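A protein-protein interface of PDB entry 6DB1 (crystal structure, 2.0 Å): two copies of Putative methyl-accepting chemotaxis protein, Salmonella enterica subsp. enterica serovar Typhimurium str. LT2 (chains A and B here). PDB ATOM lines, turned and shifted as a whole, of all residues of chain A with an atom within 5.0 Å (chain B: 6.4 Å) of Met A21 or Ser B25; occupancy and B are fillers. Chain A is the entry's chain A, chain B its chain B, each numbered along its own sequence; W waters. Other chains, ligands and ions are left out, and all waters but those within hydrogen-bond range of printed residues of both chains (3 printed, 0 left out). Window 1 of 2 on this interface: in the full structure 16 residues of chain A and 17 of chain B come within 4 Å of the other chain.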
ATOM      1  N   LEU A  17      -4.417  -0.101   3.075  1.00  0.00           N
ATOM      2  CA  LEU A  17      -5.617  -0.669   3.702  1.00  0.00           C
ATOM      3  C   LEU A  17      -5.404  -0.750   5.218  1.00  0.00           C
ATOM      4  O   LEU A  17      -6.250  -0.324   5.998  1.00  0.00           O
ATOM      5  CB  LEU A  17      -5.898  -2.071   3.154  1.00  0.00           C
ATOM      6  CG  LEU A  17      -6.471  -2.161   1.746  1.00  0.00           C
ATOM      7  CD1 LEU A  17      -6.554  -3.613   1.300  1.00  0.00           C
ATOM      8  CD2 LEU A  17      -7.840  -1.506   1.672  1.00  0.00           C
ATOM      9  N   VAL A  18      -4.255  -1.290   5.608  1.00  0.00           N
ATOM     10  CA  VAL A  18      -3.932  -1.467   7.032  1.00  0.00           C
ATOM     11  C   VAL A  18      -3.929  -0.099   7.759  1.00  0.00           C
ATOM     12  O   VAL A  18      -4.428  -0.023   8.892  1.00  0.00           O
ATOM     13  CB  VAL A  18      -2.611  -2.239   7.191  1.00  0.00           C
ATOM     14  CG1 VAL A  18      -2.138  -2.308   8.633  1.00  0.00           C
ATOM     15  CG2 VAL A  18      -2.734  -3.633   6.610  1.00  0.00           C
ATOM     16  N   ARG A  19      -3.399   0.965   7.149  1.00  0.00           N
ATOM     17  CA  ARG A  19      -3.443   2.281   7.806  1.00  0.00           C
ATOM     18  C   ARG A  19      -4.913   2.676   8.015  1.00  0.00           C
ATOM     19  O   ARG A  19      -5.275   3.162   9.057  1.00  0.00           O
ATOM     20  CB  ARG A  19      -2.696   3.359   7.004  1.00  0.00           C
ATOM     21  CG  ARG A  19      -1.173   3.285   7.077  1.00  0.00           C
ATOM     22  CD  ARG A  19      -0.456   4.436   6.375  1.00  0.00           C
ATOM     23  NE  ARG A  19      -0.410   4.325   4.913  1.00  0.00           N
ATOM     24  CZ  ARG A  19       0.667   3.993   4.207  1.00  0.00           C
ATOM     25  NH1 ARG A  19       0.568   3.832   2.899  1.00  0.00           N
ATOM     26  NH2 ARG A  19       1.838   3.835   4.803  1.00  0.00           N
ATOM     27  N   GLN A  20      -5.763   2.448   7.019  1.00  0.00           N
ATOM     28  CA  GLN A  20      -7.194   2.779   7.144  1.00  0.00           C
ATOM     29  C   GLN A  20      -7.865   1.948   8.248  1.00  0.00           C
ATOM     30  O   GLN A  20      -8.674   2.481   9.011  1.00  0.00           O
ATOM     31  CB  GLN A  20      -7.946   2.525   5.835  1.00  0.00           C
ATOM     32  CG  GLN A  20      -7.689   3.533   4.726  1.00  0.00           C
ATOM     33  CD  GLN A  20      -8.358   3.077   3.445  1.00  0.00           C
ATOM     34  OE1 GLN A  20      -7.906   2.147   2.784  1.00  0.00           O
ATOM     35  NE2 GLN A  20      -9.429   3.737   3.064  1.00  0.00           N
ATOM     36  N   MET A  21      -7.556   0.648   8.299  1.00  0.00           N
ATOM     37  CA  MET A  21      -8.139  -0.257   9.307  1.00  0.00           C
ATOM     38  C   MET A  21      -7.692   0.156  10.699  1.00  0.00           C
ATOM     39  O   MET A  21      -8.457   0.090  11.641  1.00  0.00           O
ATOM     40  CB  MET A  21      -7.786  -1.725   8.977  1.00  0.00           C
ATOM     41  CG  MET A  21      -8.273  -2.717  10.045  1.00  0.00           C
ATOM     42  SD  MET A  21      -7.746  -4.569   9.580  1.00  0.00           S
ATOM     43  CE  MET A  21      -7.552  -4.236   7.646  1.00  0.00           C
ATOM     44  N   THR A  22      -6.449   0.618  10.816  1.00  0.00           N
ATOM     45  CA  THR A  22      -5.890   1.059  12.092  1.00  0.00           C
ATOM     46  C   THR A  22      -6.532   2.377  12.538  1.00  0.00           C
ATOM     47  O   THR A  22      -6.868   2.516  13.697  1.00  0.00           O
ATOM     48  CB  THR A  22      -4.364   1.199  12.006  1.00  0.00           C
ATOM     49  OG1 THR A  22      -3.828  -0.116  11.849  1.00  0.00           O
ATOM     50  CG2 THR A  22      -3.764   1.861  13.228  1.00  0.00           C
ATOM     51  N   VAL A  23      -6.699   3.331  11.618  1.00  0.00           N
ATOM     52  CA  VAL A  23      -7.325   4.612  11.959  1.00  0.00           C
ATOM     53  C   VAL A  23      -8.789   4.385  12.372  1.00  0.00           C
ATOM     54  O   VAL A  23      -9.285   5.035  13.304  1.00  0.00           O
ATOM     55  CB  VAL A  23      -7.192   5.619  10.805  1.00  0.00           C
ATOM     56  CG1 VAL A  23      -8.074   6.845  10.992  1.00  0.00           C
ATOM     57  CG2 VAL A  23      -5.742   6.026  10.621  1.00  0.00           C
ATOM     58  N   LEU A  24      -9.478   3.481  11.689  1.00  0.00           N
ATOM     59  CA  LEU A  24     -10.866   3.163  12.017  1.00  0.00           C
ATOM     60  C   LEU A  24     -10.941   2.529  13.419  1.00  0.00           C
ATOM     61  O   LEU A  24     -11.821   2.864  14.206  1.00  0.00           O
ATOM     62  CB  LEU A  24     -11.435   2.235  10.933  1.00  0.00           C
ATOM     63  CG  LEU A  24     -12.874   1.747  11.139  1.00  0.00           C
ATOM     64  CD1 LEU A  24     -13.857   2.905  11.248  1.00  0.00           C
ATOM     65  CD2 LEU A  24     -13.288   0.801  10.011  1.00  0.00           C
ATOM     66  N   SER A  25     -10.041   1.605  13.741  1.00  0.00           N
ATOM     67  CA  SER A  25     -10.042   0.973  15.079  1.00  0.00           C
ATOM     68  C   SER A  25      -9.742   2.000  16.173  1.00  0.00           C
ATOM     69  O   SER A  25     -10.319   1.963  17.244  1.00  0.00           O
ATOM     70  CB  SER A  25      -9.060  -0.150  15.155  1.00  0.00           C
ATOM     71  OG  SER A  25      -9.494  -1.235  14.372  1.00  0.00           O
ATOM     72  N   PHE A 135     -16.757  -2.280   6.294  1.00  0.00           N
ATOM     73  CA  PHE A 135     -15.378  -1.961   5.932  1.00  0.00           C
ATOM     74  C   PHE A 135     -14.434  -3.129   6.257  1.00  0.00           C
ATOM     75  O   PHE A 135     -13.649  -3.568   5.415  1.00  0.00           O
ATOM     76  CB  PHE A 135     -14.907  -0.722   6.698  1.00  0.00           C
ATOM     77  CG  PHE A 135     -13.517  -0.282   6.321  1.00  0.00           C
ATOM     78  CD1 PHE A 135     -12.409  -0.909   6.859  1.00  0.00           C
ATOM     79  CD2 PHE A 135     -13.328   0.722   5.385  1.00  0.00           C
ATOM     80  CE1 PHE A 135     -11.131  -0.543   6.467  1.00  0.00           C
ATOM     81  CE2 PHE A 135     -12.052   1.089   4.998  1.00  0.00           C
ATOM     82  CZ  PHE A 135     -10.958   0.452   5.540  1.00  0.00           C
ATOM     83  N   ALA A 139     -12.151  -5.260   3.585  1.00  0.00           N
ATOM     84  CA  ALA A 139     -10.686  -5.179   3.767  1.00  0.00           C
ATOM     85  C   ALA A 139     -10.125  -6.577   3.998  1.00  0.00           C
ATOM     86  O   ALA A 139      -9.096  -6.947   3.423  1.00  0.00           O
ATOM     87  CB  ALA A 139     -10.339  -4.272   4.919  1.00  0.00           C
ATOM     88  N   LEU A 143      -7.275  -8.310   1.755  1.00  0.00           N
ATOM     89  CA  LEU A 143      -6.012  -8.690   2.423  1.00  0.00           C
ATOM     90  C   LEU A 143      -5.788 -10.204   2.458  1.00  0.00           C
ATOM     91  O   LEU A 143      -4.644 -10.636   2.255  1.00  0.00           O
ATOM     92  CB  LEU A 143      -6.003  -8.127   3.847  1.00  0.00           C
ATOM     93  CG  LEU A 143      -5.785  -6.619   3.938  1.00  0.00           C
ATOM     94  CD1 LEU A 143      -6.138  -6.095   5.319  1.00  0.00           C
ATOM     95  CD2 LEU A 143      -4.349  -6.256   3.564  1.00  0.00           C
ATOM     96  N   GLN B  20       2.984  -8.827   9.330  1.00  0.00           N
ATOM     97  CA  GLN B  20       2.886  -8.689  10.799  1.00  0.00           C
ATOM     98  C   GLN B  20       1.986  -7.495  11.133  1.00  0.00           C
ATOM     99  O   GLN B  20       1.093  -7.618  11.971  1.00  0.00           O
ATOM    100  CB  GLN B  20       4.262  -8.530  11.456  1.00  0.00           C
ATOM    101  CG  GLN B  20       5.093  -9.807  11.457  1.00  0.00           C
ATOM    102  CD  GLN B  20       6.464  -9.585  12.045  1.00  0.00           C
ATOM    103  OE1 GLN B  20       7.209  -8.712  11.616  1.00  0.00           O
ATOM    104  NE2 GLN B  20       6.810 -10.394  13.035  1.00  0.00           N
ATOM    105  N   MET B  21       2.196  -6.365  10.457  1.00  0.00           N
ATOM    106  CA  MET B  21       1.367  -5.180  10.657  1.00  0.00           C
ATOM    107  C   MET B  21      -0.086  -5.470  10.295  1.00  0.00           C
ATOM    108  O   MET B  21      -1.015  -5.008  10.963  1.00  0.00           O
ATOM    109  CB  MET B  21       1.848  -3.997   9.795  1.00  0.00           C
ATOM    110  CG  MET B  21       3.135  -3.379  10.306  1.00  0.00           C
ATOM    111  SD  MET B  21       3.799  -2.206   8.877  1.00  0.00           S
ATOM    112  CE  MET B  21       2.924  -0.675   9.683  1.00  0.00           C
ATOM    113  N   THR B  22      -0.284  -6.276   9.268  1.00  0.00           N
ATOM    114  CA  THR B  22      -1.631  -6.620   8.774  1.00  0.00           C
ATOM    115  C   THR B  22      -2.391  -7.479   9.805  1.00  0.00           C
ATOM    116  O   THR B  22      -3.518  -7.143  10.210  1.00  0.00           O
ATOM    117  CB  THR B  22      -1.568  -7.362   7.432  1.00  0.00           C
ATOM    118  OG1 THR B  22      -0.920  -6.522   6.478  1.00  0.00           O
ATOM    119  CG2 THR B  22      -2.937  -7.774   6.924  1.00  0.00           C
ATOM    120  N   VAL B  23      -1.771  -8.577  10.217  1.00  0.00           N
ATOM    121  CA  VAL B  23      -2.380  -9.477  11.194  1.00  0.00           C
ATOM    122  C   VAL B  23      -2.673  -8.734  12.505  1.00  0.00           C
ATOM    123  O   VAL B  23      -3.739  -8.899  13.103  1.00  0.00           O
ATOM    124  CB  VAL B  23      -1.515 -10.731  11.420  1.00  0.00           C
ATOM    125  CG1 VAL B  23      -2.002 -11.533  12.610  1.00  0.00           C
ATOM    126  CG2 VAL B  23      -1.473 -11.599  10.175  1.00  0.00           C
ATOM    127  N   LEU B  24      -1.757  -7.894  12.928  1.00  0.00           N
ATOM    128  CA  LEU B  24      -1.909  -7.111  14.138  1.00  0.00           C
ATOM    129  C   LEU B  24      -3.129  -6.174  14.024  1.00  0.00           C
ATOM    130  O   LEU B  24      -3.967  -6.049  14.957  1.00  0.00           O
ATOM    131  CB  LEU B  24      -0.599  -6.346  14.320  1.00  0.00           C
ATOM    132  CG  LEU B  24      -0.397  -5.660  15.654  1.00  0.00           C
ATOM    133  CD1 LEU B  24      -0.609  -6.643  16.796  1.00  0.00           C
ATOM    134  CD2 LEU B  24       0.999  -5.064  15.701  1.00  0.00           C
ATOM    135  N   SER B  25      -3.254  -5.507  12.886  1.00  0.00           N
ATOM    136  CA  SER B  25      -4.410  -4.641  12.634  1.00  0.00           C
ATOM    137  C   SER B  25      -5.716  -5.458  12.582  1.00  0.00           C
ATOM    138  O   SER B  25      -6.775  -4.977  13.011  1.00  0.00           O
ATOM    139  CB  SER B  25      -4.205  -3.878  11.350  1.00  0.00           C
ATOM    140  OG  SER B  25      -5.338  -3.083  11.025  1.00  0.00           O
ATOM    141  N   GLN B  26      -5.659  -6.641  11.968  1.00  0.00           N
ATOM    142  CA  GLN B  26      -6.829  -7.530  11.819  1.00  0.00           C
ATOM    143  C   GLN B  26      -7.283  -8.055  13.187  1.00  0.00           C
ATOM    144  O   GLN B  26      -8.497  -8.191  13.448  1.00  0.00           O
ATOM    145  CB  GLN B  26      -6.514  -8.713  10.905  1.00  0.00           C
ATOM    146  CG  GLN B  26      -6.558  -8.365   9.431  1.00  0.00           C
ATOM    147  CD  GLN B  26      -6.116  -9.518   8.570  1.00  0.00           C
ATOM    148  OE1 GLN B  26      -5.087 -10.142   8.819  1.00  0.00           O
ATOM    149  NE2 GLN B  26      -6.876  -9.786   7.524  1.00  0.00           N
ATOM    150  N   GLY B  27      -6.321  -8.367  14.042  1.00  0.00           N
ATOM    151  CA  GLY B  27      -6.640  -8.817  15.368  1.00  0.00           C
ATOM    152  C   GLY B  27      -7.324  -7.731  16.179  1.00  0.00           C
ATOM    153  O   GLY B  27      -8.265  -8.006  16.922  1.00  0.00           O
ATOM    154  N   ASN B  28      -6.841  -6.493  16.052  1.00  0.00           N
ATOM    155  CA  ASN B  28      -7.399  -5.397  16.807  1.00  0.00           C
ATOM    156  C   ASN B  28      -8.809  -5.090  16.280  1.00  0.00           C
ATOM    157  O   ASN B  28      -9.707  -4.736  17.030  1.00  0.00           O
ATOM    158  CB  ASN B  28      -6.487  -4.171  16.756  1.00  0.00           C
ATOM    159  CG  ASN B  28      -6.813  -3.160  17.828  1.00  0.00           C
ATOM    160  OD1 ASN B  28      -7.216  -3.527  18.933  1.00  0.00           O
ATOM    161  ND2 ASN B  28      -6.607  -1.890  17.525  1.00  0.00           N
ATOM    162  N   ASP B  29      -8.992  -5.214  14.977  1.00  0.00           N
ATOM    163  CA  ASP B  29     -10.279  -4.978  14.346  1.00  0.00           C
ATOM    164  C   ASP B  29     -11.295  -6.031  14.832  1.00  0.00           C
ATOM    165  O   ASP B  29     -12.432  -5.704  15.187  1.00  0.00           O
ATOM    166  CB  ASP B  29     -10.103  -5.027  12.821  1.00  0.00           C
ATOM    167  CG  ASP B  29     -11.410  -4.947  12.074  1.00  0.00           C
ATOM    168  OD1 ASP B  29     -12.075  -3.892  12.154  1.00  0.00           O
ATOM    169  OD2 ASP B  29     -11.748  -5.933  11.370  1.00  0.00           O
ATOM    170  N   GLN B  30     -10.884  -7.292  14.863  1.00  0.00           N
ATOM    171  CA  GLN B  30     -11.771  -8.376  15.332  1.00  0.00           C
ATOM    172  C   GLN B  30     -12.175  -8.134  16.789  1.00  0.00           C
ATOM    173  O   GLN B  30     -13.278  -8.468  17.167  1.00  0.00           O
ATOM    174  CB  GLN B  30     -11.123  -9.737  15.130  1.00  0.00           C
ATOM    175  CG  GLN B  30     -11.037 -10.090  13.657  1.00  0.00           C
ATOM    176  CD  GLN B  30     -12.410 -10.150  13.036  1.00  0.00           C
ATOM    177  OE1 GLN B  30     -13.315 -10.834  13.527  1.00  0.00           O
ATOM    178  NE2 GLN B  30     -12.568  -9.440  11.930  1.00  0.00           N
ATOM    179  N   TRP B  90      -1.587  -9.939  23.588  1.00  0.00           N
ATOM    180  CA  TRP B  90      -2.700 -10.412  22.796  1.00  0.00           C
ATOM    181  C   TRP B  90      -3.318 -11.622  23.519  1.00  0.00           C
ATOM    182  O   TRP B  90      -4.536 -11.708  23.709  1.00  0.00           O
ATOM    183  CB  TRP B  90      -2.229 -10.770  21.399  1.00  0.00           C
ATOM    184  CG  TRP B  90      -3.304 -10.927  20.372  1.00  0.00           C
ATOM    185  CD1 TRP B  90      -4.564 -11.431  20.533  1.00  0.00           C
ATOM    186  CD2 TRP B  90      -3.127 -10.759  18.958  1.00  0.00           C
ATOM    187  NE1 TRP B  90      -5.209 -11.509  19.323  1.00  0.00           N
ATOM    188  CE2 TRP B  90      -4.345 -11.106  18.339  1.00  0.00           C
ATOM    189  CE3 TRP B  90      -2.066 -10.320  18.162  1.00  0.00           C
ATOM    190  CZ2 TRP B  90      -4.515 -11.054  16.961  1.00  0.00           C
ATOM    191  CZ3 TRP B  90      -2.245 -10.245  16.801  1.00  0.00           C
ATOM    192  CH2 TRP B  90      -3.450 -10.609  16.208  1.00  0.00           C
ATOM    193  N   SER B 136       3.923  -1.181  15.191  1.00  0.00           N
ATOM    194  CA  SER B 136       3.644  -0.615  13.876  1.00  0.00           C
ATOM    195  C   SER B 136       4.444   0.659  13.611  1.00  0.00           C
ATOM    196  O   SER B 136       4.692   0.977  12.445  1.00  0.00           O
ATOM    197  CB  SER B 136       2.170  -0.378  13.716  1.00  0.00           C
ATOM    198  OG  SER B 136       1.468  -1.602  13.889  1.00  0.00           O
HETATM  199  O   HOH W   1     -12.462  -1.267  13.912  1.00  0.00           O
HETATM  200  O   HOH W   2      -7.243  -2.184  13.433  1.00  0.00           O
HETATM  201  O   HOH W   3     -10.799  -1.247  11.694  1.00  0.00           O
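The side-chain sulfur of Met A21 sits close to the side-chain hydroxyl of Ser B25 (3.2 Å).
The side-chain sulfur (SD) of Met A21 sits at hydrogen-bond distance from the backbone NH (N) of Gln B26, at 3.8 Å.
The side-chain hydroxyl (OG) of Ser B25 is in hydrogen-bond range of the side-chain hydroxyl (OG1) of Thr A22, 3.4 Å away.
The side-chain hydroxyl of Thr A22 sits at hydrogen-bond distance from the backbone carbonyl oxygen of Val A18, 3.0 Å away.
O of Met A21 sits at hydrogen-bond distance from OG of Ser A25.
Among the printed residues, merely in contact across the chains: Val A18 with Thr B22 (3.4 Å), Val A18 with Met B21 (3.7 Å), Val A18 with Ser B25 (3.8 Å), Ser A25 with Asp B29 (3.8 Å), Ser A25 with Asn B28 (3.8 Å) and Leu A143 with Thr B22 (3.9 Å).
Printed residues of chain B within 4 Å of Met A21: Ser B25 and Gln B26.
Printed residues of chain A within 4 Å of Ser B25: Val A18 (3.8 Å), Met A21 (3.1 Å) and Thr A22 (3.4 Å).
Of the printed residues of chain B, Thr A22 touches Ser B25.
Printed residues of chain A within 4 Å of Asn B28: Ser A25.
Of the printed residues of chain A, Asp B29 touches Ser A25.
Val A23 touches none of the printed residues of chain B.
The nearest printed residue of chain A that does not touch Gln B26 is Leu A143 (4.1 Å).
Along chain B the printed residues that touch a printed residue of chain A span positions 21 to 29.
Hydrophobic or aromatic side chains of chain A that line the printed part of chain B: Val A18, Met A21 and Leu A143.
Met A21 touches Ser B25, but with the chains exchanged Ser A25 does not touch Met B21 (9.9 Å).
Thr A22 touches Ser B25, but with the chains exchanged Ser A25 does not touch Thr B22 (9.4 Å).
Of the 9 pairs that touch across the chains among the printed residues, none has its exchanged pair printed and touching as well.
Water W2 lies within hydrogen-bond range of OG of Ser A25 (2.6 Å), O of Ser B25 (2.9 Å) and O of Met A21 (3.1 Å).
Water W3 lies within hydrogen-bond range of O of Met A21 (2.7 Å), OD1 of Asp B29 (3.0 Å) and OG of Ser A25 (3.0 Å).
Water W1 bridges the side-chain hydroxyl of Ser A25 (3.0 Å) and the side-chain carboxylate of Asp B29 (3.2 Å).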
